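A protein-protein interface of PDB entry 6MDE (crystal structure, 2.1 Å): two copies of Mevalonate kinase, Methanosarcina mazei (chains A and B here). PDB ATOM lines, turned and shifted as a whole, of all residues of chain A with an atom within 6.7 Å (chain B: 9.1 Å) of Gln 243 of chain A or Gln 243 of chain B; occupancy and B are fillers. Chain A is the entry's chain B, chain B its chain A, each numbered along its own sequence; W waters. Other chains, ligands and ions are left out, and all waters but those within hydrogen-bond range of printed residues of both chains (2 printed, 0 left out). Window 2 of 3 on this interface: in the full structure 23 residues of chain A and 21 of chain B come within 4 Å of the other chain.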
ATOM      1  N   ILE A 238      23.702  33.100 -16.300  1.00  0.00           N
ATOM      2  CA  ILE A 238      24.179  32.105 -15.338  1.00  0.00           C
ATOM      3  C   ILE A 238      24.033  30.719 -15.949  1.00  0.00           C
ATOM      4  O   ILE A 238      23.397  30.541 -16.979  1.00  0.00           O
ATOM      5  CB  ILE A 238      23.432  32.162 -13.978  1.00  0.00           C
ATOM      6  CG1 ILE A 238      21.963  31.671 -14.122  1.00  0.00           C
ATOM      7  CG2 ILE A 238      23.573  33.545 -13.330  1.00  0.00           C
ATOM      8  CD1 ILE A 238      21.158  31.633 -12.773  1.00  0.00           C
ATOM      9  N   LEU A 239      24.586  29.728 -15.243  1.00  0.00           N
ATOM     10  CA  LEU A 239      24.604  28.356 -15.727  1.00  0.00           C
ATOM     11  C   LEU A 239      23.197  27.834 -15.991  1.00  0.00           C
ATOM     12  O   LEU A 239      22.942  27.232 -17.038  1.00  0.00           O
ATOM     13  CB  LEU A 239      25.328  27.473 -14.710  1.00  0.00           C
ATOM     14  CG  LEU A 239      25.243  25.951 -14.871  1.00  0.00           C
ATOM     15  CD1 LEU A 239      26.031  25.454 -16.072  1.00  0.00           C
ATOM     16  CD2 LEU A 239      25.702  25.251 -13.595  1.00  0.00           C
ATOM     17  N   GLU A 240      22.258  28.104 -15.076  1.00  0.00           N
ATOM     18  CA  GLU A 240      20.923  27.540 -15.223  1.00  0.00           C
ATOM     19  C   GLU A 240      20.191  28.148 -16.410  1.00  0.00           C
ATOM     20  O   GLU A 240      19.489  27.435 -17.136  1.00  0.00           O
ATOM     21  CB  GLU A 240      20.119  27.720 -13.932  1.00  0.00           C
ATOM     22  CG  GLU A 240      20.589  26.857 -12.791  1.00  0.00           C
ATOM     23  CD  GLU A 240      21.602  27.574 -11.893  1.00  0.00           C
ATOM     24  OE1 GLU A 240      22.347  28.489 -12.355  1.00  0.00           O
ATOM     25  OE2 GLU A 240      21.653  27.219 -10.705  1.00  0.00           O
ATOM     26  N   LEU A 241      20.340  29.462 -16.632  1.00  0.00           N
ATOM     27  CA  LEU A 241      19.775  30.064 -17.841  1.00  0.00           C
ATOM     28  C   LEU A 241      20.370  29.438 -19.094  1.00  0.00           C
ATOM     29  O   LEU A 241      19.657  29.206 -20.078  1.00  0.00           O
ATOM     30  CB  LEU A 241      20.024  31.582 -17.862  1.00  0.00           C
ATOM     31  CG  LEU A 241      19.209  32.434 -16.886  1.00  0.00           C
ATOM     32  CD1 LEU A 241      19.698  33.882 -16.827  1.00  0.00           C
ATOM     33  CD2 LEU A 241      17.756  32.380 -17.242  1.00  0.00           C
ATOM     34  N   SER A 242      21.689  29.191 -19.087  1.00  0.00           N
ATOM     35  CA  SER A 242      22.342  28.654 -20.281  1.00  0.00           C
ATOM     36  C   SER A 242      21.863  27.249 -20.580  1.00  0.00           C
ATOM     37  O   SER A 242      21.643  26.894 -21.743  1.00  0.00           O
ATOM     38  CB  SER A 242      23.867  28.639 -20.109  1.00  0.00           C
ATOM     39  OG  SER A 242      24.417  29.874 -20.470  1.00  0.00           O
ATOM     40  N   GLN A 243      21.732  26.421 -19.543  1.00  0.00           N
ATOM     41  CA  GLN A 243      21.254  25.059 -19.763  1.00  0.00           C
ATOM     42  C   GLN A 243      19.871  25.073 -20.399  1.00  0.00           C
ATOM     43  O   GLN A 243      19.603  24.344 -21.364  1.00  0.00           O
ATOM     44  CB  GLN A 243      21.241  24.306 -18.433  1.00  0.00           C
ATOM     45  CG  GLN A 243      22.633  24.102 -17.885  1.00  0.00           C
ATOM     46  CD  GLN A 243      22.626  23.549 -16.491  1.00  0.00           C
ATOM     47  OE1 GLN A 243      21.800  23.931 -15.666  1.00  0.00           O
ATOM     48  NE2 GLN A 243      23.550  22.641 -16.212  1.00  0.00           N
ATOM     49  N   LEU A 244      18.988  25.932 -19.896  1.00  0.00           N
ATOM     50  CA  LEU A 244      17.641  25.970 -20.452  1.00  0.00           C
ATOM     51  C   LEU A 244      17.670  26.470 -21.881  1.00  0.00           C
ATOM     52  O   LEU A 244      16.974  25.937 -22.753  1.00  0.00           O
ATOM     53  CB  LEU A 244      16.734  26.855 -19.598  1.00  0.00           C
ATOM     54  CG  LEU A 244      16.553  26.495 -18.109  1.00  0.00           C
ATOM     55  CD1 LEU A 244      15.356  27.235 -17.540  1.00  0.00           C
ATOM     56  CD2 LEU A 244      16.413  24.975 -17.864  1.00  0.00           C
ATOM     57  N   ILE A 245      18.486  27.488 -22.132  1.00  0.00           N
ATOM     58  CA  ILE A 245      18.553  28.088 -23.453  1.00  0.00           C
ATOM     59  C   ILE A 245      19.073  27.070 -24.473  1.00  0.00           C
ATOM     60  O   ILE A 245      18.479  26.874 -25.539  1.00  0.00           O
ATOM     61  CB  ILE A 245      19.422  29.358 -23.391  1.00  0.00           C
ATOM     62  CG1 ILE A 245      18.633  30.508 -22.742  1.00  0.00           C
ATOM     63  CG2 ILE A 245      19.972  29.743 -24.778  1.00  0.00           C
ATOM     64  CD1 ILE A 245      19.508  31.685 -22.260  1.00  0.00           C
ATOM     65  N   TYR A 246      20.181  26.393 -24.156  1.00  0.00           N
ATOM     66  CA  TYR A 246      20.734  25.455 -25.128  1.00  0.00           C
ATOM     67  C   TYR A 246      19.841  24.232 -25.294  1.00  0.00           C
ATOM     68  O   TYR A 246      19.759  23.681 -26.393  1.00  0.00           O
ATOM     69  CB  TYR A 246      22.173  25.069 -24.755  1.00  0.00           C
ATOM     70  CG  TYR A 246      23.144  26.118 -25.272  1.00  0.00           C
ATOM     71  CD1 TYR A 246      23.359  26.273 -26.639  1.00  0.00           C
ATOM     72  CD2 TYR A 246      23.781  26.997 -24.407  1.00  0.00           C
ATOM     73  CE1 TYR A 246      24.181  27.253 -27.139  1.00  0.00           C
ATOM     74  CE2 TYR A 246      24.635  27.987 -24.899  1.00  0.00           C
ATOM     75  CZ  TYR A 246      24.827  28.107 -26.258  1.00  0.00           C
ATOM     76  OH  TYR A 246      25.659  29.086 -26.737  1.00  0.00           O
ATOM     77  N   SER A 247      19.144  23.804 -24.234  1.00  0.00           N
ATOM     78  CA  SER A 247      18.218  22.684 -24.394  1.00  0.00           C
ATOM     79  C   SER A 247      17.083  23.048 -25.344  1.00  0.00           C
ATOM     80  O   SER A 247      16.680  22.235 -26.183  1.00  0.00           O
ATOM     81  CB  SER A 247      17.677  22.232 -23.035  1.00  0.00           C
ATOM     82  OG  SER A 247      16.528  22.958 -22.645  1.00  0.00           O
ATOM     83  N   ALA A 248      16.572  24.279 -25.252  1.00  0.00           N
ATOM     84  CA  ALA A 248      15.500  24.702 -26.151  1.00  0.00           C
ATOM     85  C   ALA A 248      15.966  24.756 -27.604  1.00  0.00           C
ATOM     86  O   ALA A 248      15.218  24.382 -28.522  1.00  0.00           O
ATOM     87  CB  ALA A 248      14.970  26.063 -25.722  1.00  0.00           C
ATOM     88  N   ALA A 282      12.008  19.644 -23.505  1.00  0.00           N
ATOM     89  CA  ALA A 282      13.459  19.719 -23.368  1.00  0.00           C
ATOM     90  C   ALA A 282      13.856  20.712 -22.271  1.00  0.00           C
ATOM     91  O   ALA A 282      14.763  20.438 -21.470  1.00  0.00           O
ATOM     92  CB  ALA A 282      14.086  20.085 -24.716  1.00  0.00           C
ATOM     93  N   VAL A 283      13.158  21.846 -22.181  1.00  0.00           N
ATOM     94  CA  VAL A 283      13.491  22.815 -21.141  1.00  0.00           C
ATOM     95  C   VAL A 283      13.211  22.233 -19.763  1.00  0.00           C
ATOM     96  O   VAL A 283      14.037  22.359 -18.847  1.00  0.00           O
ATOM     97  CB  VAL A 283      12.748  24.148 -21.364  1.00  0.00           C
ATOM     98  CG1 VAL A 283      12.907  25.065 -20.123  1.00  0.00           C
ATOM     99  CG2 VAL A 283      13.293  24.859 -22.593  1.00  0.00           C
ATOM    100  N   ALA A 286      15.870  19.796 -18.739  1.00  0.00           N
ATOM    101  CA  ALA A 286      17.078  20.489 -18.307  1.00  0.00           C
ATOM    102  C   ALA A 286      16.931  21.088 -16.915  1.00  0.00           C
ATOM    103  O   ALA A 286      17.867  21.742 -16.428  1.00  0.00           O
ATOM    104  CB  ALA A 286      17.430  21.591 -19.304  1.00  0.00           C
ATOM    105  N   GLY B 168      39.473  22.630 -19.734  1.00  0.00           N
ATOM    106  CA  GLY B 168      38.425  21.636 -19.702  1.00  0.00           C
ATOM    107  C   GLY B 168      38.002  21.224 -21.094  1.00  0.00           C
ATOM    108  O   GLY B 168      37.579  22.056 -21.905  1.00  0.00           O
ATOM    109  N   THR B 170      35.518  19.224 -23.475  1.00  0.00           N
ATOM    110  CA  THR B 170      34.163  18.697 -23.537  1.00  0.00           C
ATOM    111  C   THR B 170      34.092  17.344 -24.225  1.00  0.00           C
ATOM    112  O   THR B 170      33.039  16.705 -24.183  1.00  0.00           O
ATOM    113  CB  THR B 170      33.255  19.669 -24.280  1.00  0.00           C
ATOM    114  OG1 THR B 170      33.708  19.796 -25.632  1.00  0.00           O
ATOM    115  CG2 THR B 170      33.266  21.039 -23.621  1.00  0.00           C
ATOM    116  N   GLN B 228      34.030  35.731 -23.829  1.00  0.00           N
ATOM    117  CA  GLN B 228      33.231  34.522 -23.952  1.00  0.00           C
ATOM    118  C   GLN B 228      31.826  34.855 -24.435  1.00  0.00           C
ATOM    119  O   GLN B 228      31.284  34.166 -25.308  1.00  0.00           O
ATOM    120  CB  GLN B 228      33.194  33.779 -22.619  1.00  0.00           C
ATOM    121  CG  GLN B 228      32.210  32.572 -22.607  1.00  0.00           C
ATOM    122  CD  GLN B 228      32.542  31.528 -23.674  1.00  0.00           C
ATOM    123  OE1 GLN B 228      33.688  31.436 -24.153  1.00  0.00           O
ATOM    124  NE2 GLN B 228      31.543  30.721 -24.042  1.00  0.00           N
ATOM    125  N   ASN B 237      29.516  28.800 -29.231  1.00  0.00           N
ATOM    126  CA  ASN B 237      29.417  28.167 -27.925  1.00  0.00           C
ATOM    127  C   ASN B 237      28.461  26.962 -27.973  1.00  0.00           C
ATOM    128  O   ASN B 237      27.577  26.894 -28.829  1.00  0.00           O
ATOM    129  CB  ASN B 237      28.954  29.194 -26.899  1.00  0.00           C
ATOM    130  CG  ASN B 237      29.188  28.732 -25.498  1.00  0.00           C
ATOM    131  OD1 ASN B 237      30.041  27.873 -25.256  1.00  0.00           O
ATOM    132  ND2 ASN B 237      28.424  29.284 -24.552  1.00  0.00           N
ATOM    133  N   ILE B 238      28.659  25.990 -27.066  1.00  0.00           N
ATOM    134  CA  ILE B 238      27.723  24.865 -26.917  1.00  0.00           C
ATOM    135  C   ILE B 238      27.454  24.607 -25.437  1.00  0.00           C
ATOM    136  O   ILE B 238      28.150  25.114 -24.553  1.00  0.00           O
ATOM    137  CB  ILE B 238      28.205  23.556 -27.590  1.00  0.00           C
ATOM    138  CG1 ILE B 238      29.386  22.939 -26.824  1.00  0.00           C
ATOM    139  CG2 ILE B 238      28.498  23.768 -29.066  1.00  0.00           C
ATOM    140  CD1 ILE B 238      29.733  21.507 -27.261  1.00  0.00           C
ATOM    141  N   LEU B 239      26.414  23.801 -25.178  1.00  0.00           N
ATOM    142  CA  LEU B 239      25.993  23.531 -23.804  1.00  0.00           C
ATOM    143  C   LEU B 239      27.147  23.033 -22.945  1.00  0.00           C
ATOM    144  O   LEU B 239      27.369  23.524 -21.830  1.00  0.00           O
ATOM    145  CB  LEU B 239      24.860  22.505 -23.788  1.00  0.00           C
ATOM    146  CG  LEU B 239      24.649  21.879 -22.401  1.00  0.00           C
ATOM    147  CD1 LEU B 239      24.116  22.926 -21.401  1.00  0.00           C
ATOM    148  CD2 LEU B 239      23.740  20.641 -22.452  1.00  0.00           C
ATOM    149  N   GLU B 240      27.889  22.046 -23.452  1.00  0.00           N
ATOM    150  CA  GLU B 240      29.001  21.482 -22.694  1.00  0.00           C
ATOM    151  C   GLU B 240      30.047  22.538 -22.351  1.00  0.00           C
ATOM    152  O   GLU B 240      30.590  22.544 -21.239  1.00  0.00           O
ATOM    153  CB  GLU B 240      29.627  20.333 -23.484  1.00  0.00           C
ATOM    154  CG  GLU B 240      28.760  19.098 -23.547  1.00  0.00           C
ATOM    155  CD  GLU B 240      27.657  19.197 -24.578  1.00  0.00           C
ATOM    156  OE1 GLU B 240      27.556  20.236 -25.270  1.00  0.00           O
ATOM    157  OE2 GLU B 240      26.879  18.230 -24.694  1.00  0.00           O
ATOM    158  N   LEU B 241      30.342  23.447 -23.288  1.00  0.00           N
ATOM    159  CA  LEU B 241      31.329  24.486 -22.999  1.00  0.00           C
ATOM    160  C   LEU B 241      30.818  25.414 -21.897  1.00  0.00           C
ATOM    161  O   LEU B 241      31.537  25.704 -20.939  1.00  0.00           O
ATOM    162  CB  LEU B 241      31.676  25.272 -24.281  1.00  0.00           C
ATOM    163  CG  LEU B 241      32.549  24.563 -25.332  1.00  0.00           C
ATOM    164  CD1 LEU B 241      32.611  25.328 -26.675  1.00  0.00           C
ATOM    165  CD2 LEU B 241      33.951  24.319 -24.770  1.00  0.00           C
ATOM    166  N   SER B 242      29.576  25.887 -22.023  1.00  0.00           N
ATOM    167  CA  SER B 242      28.969  26.712 -20.976  1.00  0.00           C
ATOM    168  C   SER B 242      29.096  26.074 -19.602  1.00  0.00           C
ATOM    169  O   SER B 242      29.470  26.740 -18.633  1.00  0.00           O
ATOM    170  CB  SER B 242      27.495  26.975 -21.284  1.00  0.00           C
ATOM    171  OG  SER B 242      27.339  28.175 -22.012  1.00  0.00           O
ATOM    172  N   GLN B 243      28.786  24.778 -19.501  1.00  0.00           N
ATOM    173  CA  GLN B 243      28.780  24.130 -18.193  1.00  0.00           C
ATOM    174  C   GLN B 243      30.166  24.117 -17.574  1.00  0.00           C
ATOM    175  O   GLN B 243      30.315  24.385 -16.371  1.00  0.00           O
ATOM    176  CB  GLN B 243      28.220  22.706 -18.301  1.00  0.00           C
ATOM    177  CG  GLN B 243      26.736  22.707 -18.708  1.00  0.00           C
ATOM    178  CD  GLN B 243      26.115  21.316 -18.852  1.00  0.00           C
ATOM    179  OE1 GLN B 243      24.991  21.104 -18.413  1.00  0.00           O
ATOM    180  NE2 GLN B 243      26.824  20.384 -19.496  1.00  0.00           N
ATOM    181  N   LEU B 244      31.191  23.777 -18.371  1.00  0.00           N
ATOM    182  CA  LEU B 244      32.566  23.814 -17.883  1.00  0.00           C
ATOM    183  C   LEU B 244      32.932  25.219 -17.443  1.00  0.00           C
ATOM    184  O   LEU B 244      33.471  25.419 -16.346  1.00  0.00           O
ATOM    185  CB  LEU B 244      33.543  23.319 -18.965  1.00  0.00           C
ATOM    186  CG  LEU B 244      33.319  21.905 -19.513  1.00  0.00           C
ATOM    187  CD1 LEU B 244      34.608  21.345 -20.169  1.00  0.00           C
ATOM    188  CD2 LEU B 244      32.763  20.958 -18.438  1.00  0.00           C
ATOM    189  N   ILE B 245      32.587  26.208 -18.273  1.00  0.00           N
ATOM    190  CA  ILE B 245      32.966  27.600 -18.026  1.00  0.00           C
ATOM    191  C   ILE B 245      32.282  28.135 -16.769  1.00  0.00           C
ATOM    192  O   ILE B 245      32.914  28.770 -15.914  1.00  0.00           O
ATOM    193  CB  ILE B 245      32.609  28.459 -19.250  1.00  0.00           C
ATOM    194  CG1 ILE B 245      33.579  28.198 -20.412  1.00  0.00           C
ATOM    195  CG2 ILE B 245      32.603  29.931 -18.868  1.00  0.00           C
ATOM    196  CD1 ILE B 245      33.050  28.690 -21.729  1.00  0.00           C
ATOM    197  N   TYR B 246      30.974  27.926 -16.651  1.00  0.00           N
ATOM    198  CA  TYR B 246      30.298  28.425 -15.455  1.00  0.00           C
ATOM    199  C   TYR B 246      30.765  27.681 -14.213  1.00  0.00           C
ATOM    200  O   TYR B 246      30.920  28.288 -13.143  1.00  0.00           O
ATOM    201  CB  TYR B 246      28.788  28.359 -15.646  1.00  0.00           C
ATOM    202  CG  TYR B 246      28.327  29.616 -16.327  1.00  0.00           C
ATOM    203  CD1 TYR B 246      28.313  30.819 -15.645  1.00  0.00           C
ATOM    204  CD2 TYR B 246      27.985  29.620 -17.662  1.00  0.00           C
ATOM    205  CE1 TYR B 246      27.926  31.981 -16.266  1.00  0.00           C
ATOM    206  CE2 TYR B 246      27.605  30.782 -18.294  1.00  0.00           C
ATOM    207  CZ  TYR B 246      27.571  31.957 -17.592  1.00  0.00           C
ATOM    208  OH  TYR B 246      27.194  33.132 -18.210  1.00  0.00           O
ATOM    209  N   SER B 247      31.036  26.379 -14.336  1.00  0.00           N
ATOM    210  CA  SER B 247      31.535  25.638 -13.183  1.00  0.00           C
ATOM    211  C   SER B 247      32.927  26.097 -12.774  1.00  0.00           C
ATOM    212  O   SER B 247      33.251  26.091 -11.581  1.00  0.00           O
ATOM    213  CB  SER B 247      31.523  24.137 -13.471  1.00  0.00           C
ATOM    214  OG  SER B 247      30.213  23.695 -13.792  1.00  0.00           O
ATOM    215  N   ALA B 248      33.768  26.501 -13.734  1.00  0.00           N
ATOM    216  CA  ALA B 248      35.078  27.025 -13.364  1.00  0.00           C
ATOM    217  C   ALA B 248      34.933  28.350 -12.644  1.00  0.00           C
ATOM    218  O   ALA B 248      35.608  28.597 -11.638  1.00  0.00           O
ATOM    219  CB  ALA B 248      35.979  27.185 -14.604  1.00  0.00           C
ATOM    220  N   ARG B 249      34.064  29.224 -13.156  1.00  0.00           N
ATOM    221  CA  ARG B 249      33.884  30.528 -12.530  1.00  0.00           C
ATOM    222  C   ARG B 249      33.402  30.381 -11.093  1.00  0.00           C
ATOM    223  O   ARG B 249      33.953  31.000 -10.174  1.00  0.00           O
ATOM    224  CB  ARG B 249      32.906  31.361 -13.348  1.00  0.00           C
ATOM    225  CG  ARG B 249      33.446  31.760 -14.704  1.00  0.00           C
ATOM    226  CD  ARG B 249      32.420  32.555 -15.447  1.00  0.00           C
ATOM    227  NE  ARG B 249      32.856  32.845 -16.802  1.00  0.00           N
ATOM    228  CZ  ARG B 249      32.041  33.256 -17.761  1.00  0.00           C
ATOM    229  NH1 ARG B 249      30.745  33.424 -17.507  1.00  0.00           N
ATOM    230  NH2 ARG B 249      32.510  33.503 -18.972  1.00  0.00           N
ATOM    231  N   ALA B 250      32.406  29.521 -10.870  1.00  0.00           N
ATOM    232  CA  ALA B 250      31.864  29.376  -9.523  1.00  0.00           C
ATOM    233  C   ALA B 250      32.903  28.819  -8.557  1.00  0.00           C
ATOM    234  O   ALA B 250      32.831  29.078  -7.349  1.00  0.00           O
ATOM    235  CB  ALA B 250      30.621  28.492  -9.550  1.00  0.00           C
ATOM    236  N   ALA B 251      33.887  28.076  -9.063  1.00  0.00           N
ATOM    237  CA  ALA B 251      34.927  27.545  -8.198  1.00  0.00           C
ATOM    238  C   ALA B 251      36.058  28.526  -7.941  1.00  0.00           C
ATOM    239  O   ALA B 251      37.028  28.152  -7.281  1.00  0.00           O
ATOM    240  CB  ALA B 251      35.499  26.254  -8.773  1.00  0.00           C
ATOM    241  N   ALA B 256      36.926  32.501 -17.499  1.00  0.00           N
ATOM    242  CA  ALA B 256      36.916  31.267 -18.257  1.00  0.00           C
ATOM    243  C   ALA B 256      36.233  31.523 -19.587  1.00  0.00           C
ATOM    244  O   ALA B 256      35.298  32.322 -19.682  1.00  0.00           O
ATOM    245  CB  ALA B 256      36.230  30.130 -17.481  1.00  0.00           C
ATOM    246  N   MET B 267      37.610  24.632 -23.159  1.00  0.00           N
ATOM    247  CA  MET B 267      37.629  25.960 -22.585  1.00  0.00           C
ATOM    248  C   MET B 267      38.870  26.096 -21.719  1.00  0.00           C
ATOM    249  O   MET B 267      39.551  25.126 -21.400  1.00  0.00           O
ATOM    250  CB  MET B 267      36.368  26.255 -21.764  1.00  0.00           C
ATOM    251  CG  MET B 267      35.907  25.105 -20.883  1.00  0.00           C
ATOM    252  SD  MET B 267      36.911  24.834 -19.412  1.00  0.00           S
ATOM    253  CE  MET B 267      36.876  26.425 -18.591  1.00  0.00           C
ATOM    254  N   VAL B 279      39.103  24.438  -8.904  1.00  0.00           N
ATOM    255  CA  VAL B 279      38.564  24.730 -10.229  1.00  0.00           C
ATOM    256  C   VAL B 279      38.555  23.469 -11.086  1.00  0.00           C
ATOM    257  O   VAL B 279      37.551  23.142 -11.727  1.00  0.00           O
ATOM    258  CB  VAL B 279      39.373  25.871 -10.877  1.00  0.00           C
ATOM    259  CG1 VAL B 279      39.119  25.941 -12.381  1.00  0.00           C
ATOM    260  CG2 VAL B 279      39.025  27.176 -10.204  1.00  0.00           C
ATOM    261  N   ALA B 282      35.714  21.117  -9.942  1.00  0.00           N
ATOM    262  CA  ALA B 282      34.401  21.575 -10.390  1.00  0.00           C
ATOM    263  C   ALA B 282      34.202  21.302 -11.871  1.00  0.00           C
ATOM    264  O   ALA B 282      33.100  20.938 -12.305  1.00  0.00           O
ATOM    265  CB  ALA B 282      34.234  23.069 -10.099  1.00  0.00           C
ATOM    266  N   VAL B 283      35.262  21.473 -12.662  1.00  0.00           N
ATOM    267  CA  VAL B 283      35.153  21.265 -14.101  1.00  0.00           C
ATOM    268  C   VAL B 283      34.971  19.790 -14.412  1.00  0.00           C
ATOM    269  O   VAL B 283      34.149  19.422 -15.258  1.00  0.00           O
ATOM    270  CB  VAL B 283      36.380  21.841 -14.831  1.00  0.00           C
ATOM    271  CG1 VAL B 283      36.348  21.418 -16.315  1.00  0.00           C
ATOM    272  CG2 VAL B 283      36.418  23.365 -14.702  1.00  0.00           C
ATOM    273  N   ALA B 284      35.745  18.922 -13.752  1.00  0.00           N
ATOM    274  CA  ALA B 284      35.533  17.484 -13.917  1.00  0.00           C
ATOM    275  C   ALA B 284      34.143  17.083 -13.442  1.00  0.00           C
ATOM    276  O   ALA B 284      33.441  16.312 -14.116  1.00  0.00           O
ATOM    277  CB  ALA B 284      36.603  16.702 -13.161  1.00  0.00           C
ATOM    278  N   GLY B 285      33.722  17.624 -12.291  1.00  0.00           N
ATOM    279  CA  GLY B 285      32.392  17.337 -11.777  1.00  0.00           C
ATOM    280  C   GLY B 285      31.297  17.703 -12.754  1.00  0.00           C
ATOM    281  O   GLY B 285      30.288  17.003 -12.860  1.00  0.00           O
ATOM    282  N   ALA B 286      31.486  18.789 -13.504  1.00  0.00           N
ATOM    283  CA  ALA B 286      30.497  19.173 -14.510  1.00  0.00           C
ATOM    284  C   ALA B 286      30.654  18.422 -15.828  1.00  0.00           C
ATOM    285  O   ALA B 286      29.957  18.754 -16.795  1.00  0.00           O
ATOM    286  CB  ALA B 286      30.551  20.685 -14.765  1.00  0.00           C
ATOM    287  N   GLY B 287      31.544  17.439 -15.903  1.00  0.00           N
ATOM    288  CA  GLY B 287      31.642  16.594 -17.072  1.00  0.00           C
ATOM    289  C   GLY B 287      32.801  16.864 -18.007  1.00  0.00           C
ATOM    290  O   GLY B 287      32.729  16.476 -19.181  1.00  0.00           O
ATOM    291  N   GLY B 288      33.863  17.504 -17.540  1.00  0.00           N
ATOM    292  CA  GLY B 288      34.975  17.889 -18.391  1.00  0.00           C
ATOM    293  C   GLY B 288      36.178  17.004 -18.122  1.00  0.00           C
ATOM    294  O   GLY B 288      36.469  16.676 -16.969  1.00  0.00           O
HETATM  295  O   HOH W   1      26.897  30.323 -29.606  1.00  0.00           O
HETATM  296  O   HOH W   2      26.150  30.959 -22.497  1.00  0.00           O
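Ile 238 of chain A touches Tyr 246 of chain B, but with the chains exchanged Tyr 246 of chain A does not touch Ile 238 of chain B (4.3 Å). Leu 239 of chain A touches Gln 243 of chain B, and with the chains exchanged Gln 243 of chain A touches Leu 239 of chain B. Leu 239 of chain A touches Tyr 246 of chain B, and with the chains exchanged Tyr 246 of chain A touches Leu 239 of chain B. Ser 242 of chain B touches its own counterpart, Ser 242 of chain A. 14 positions are printed for both chains. Of the 10 pairs that touch across the chains among the printed residues, 8 have their exchanged pair printed and touching as well.
NE2 of Gln 228 of chain B sits close to OD1 of Asn 237 of chain B, at 3.4 Å. The side-chain amide nitrogen of Asn 237 of chain B is in hydrogen-bond range of the side-chain hydroxyl of Ser 242 of chain B (3.0 Å). OG of Ser 247 of chain B is in hydrogen-bond range of O of Gln 243 of chain B, 2.7 Å away.
OE1 of Gln 243 of chain B lies within hydrogen-bond range of NE2 of Gln 243 of chain A (3.0 Å).
Among the printed residues, merely in contact across the chains: Tyr 246 of chain A with Asn 237 of chain B (3.3 Å), Leu 239 of chain A with Tyr 246 of chain B (3.7 Å), Ser 242 of chain A with Ser 242 of chain B (3.7 Å), Leu 239 of chain A with Gln 243 of chain B (3.7 Å), Tyr 246 of chain A with Leu 239 of chain B (3.8 Å), Ile 238 of chain A with Tyr 246 of chain B (3.9 Å), Gln 243 of chain A with Leu 239 of chain B (3.9 Å), Tyr 246 of chain A with Ser 242 of chain B (3.96 Å) and Ser 242 of chain A with Tyr 246 of chain B (3.97 Å).
Water W2 lies within hydrogen-bond range of OG of Ser 242 of chain A, OG of Ser 242 of chain B and ND2 of Asn 237 of chain B. Water W1 lies within hydrogen-bond range of N of Asn 237 of chain B and OH of Tyr 246 of chain A.
Of the 28 printed residues of chain B, 5 touch a printed residue of chain A. Hydrophobic or aromatic side chains of chain B that line the printed part of chain A: Leu 239 and Tyr 246. Along chain B the printed residues that touch a printed residue of chain A span positions 237 to 246. Printed residues of chain A that touch a printed residue of chain B: Ile 238, Leu 239, Ser 242, Gln 243 and Tyr 246. Among the printed residues, 10 pairs touch across the chains.
Gln 243 of chain B touches just these residues of chain A: Leu 239 (3.7 Å) and Gln 243 (3.0 Å). Of chain B, only Ser 242 (3.7 Å) and Tyr 246 (3.97 Å) come within 4 Å of Ser 242 of chain A. Printed residues of chain B within 4 Å of Leu 239 of chain A: Gln 243 and Tyr 246. Of the printed residues of chain B, Tyr 246 of chain A touches Asn 237 (3.3 Å), Leu 239 (3.8 Å) and Ser 242 (3.96 Å). Printed residues of chain B within 4 Å of Ile 238 of chain A: Tyr 246 (3.9 Å). Printed residues of chain A within 4 Å of Asn 237 of chain B: Tyr 246. Ala 250 of chain B touches none of the printed residues of chain A. The nearest residue of chain B that does not touch Gln 243 of chain A is Ser 242 of chain B (6.0 Å). The nearest residue of chain A that does not touch Gln 243 of chain B is Ser 242 of chain A (6.3 Å).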
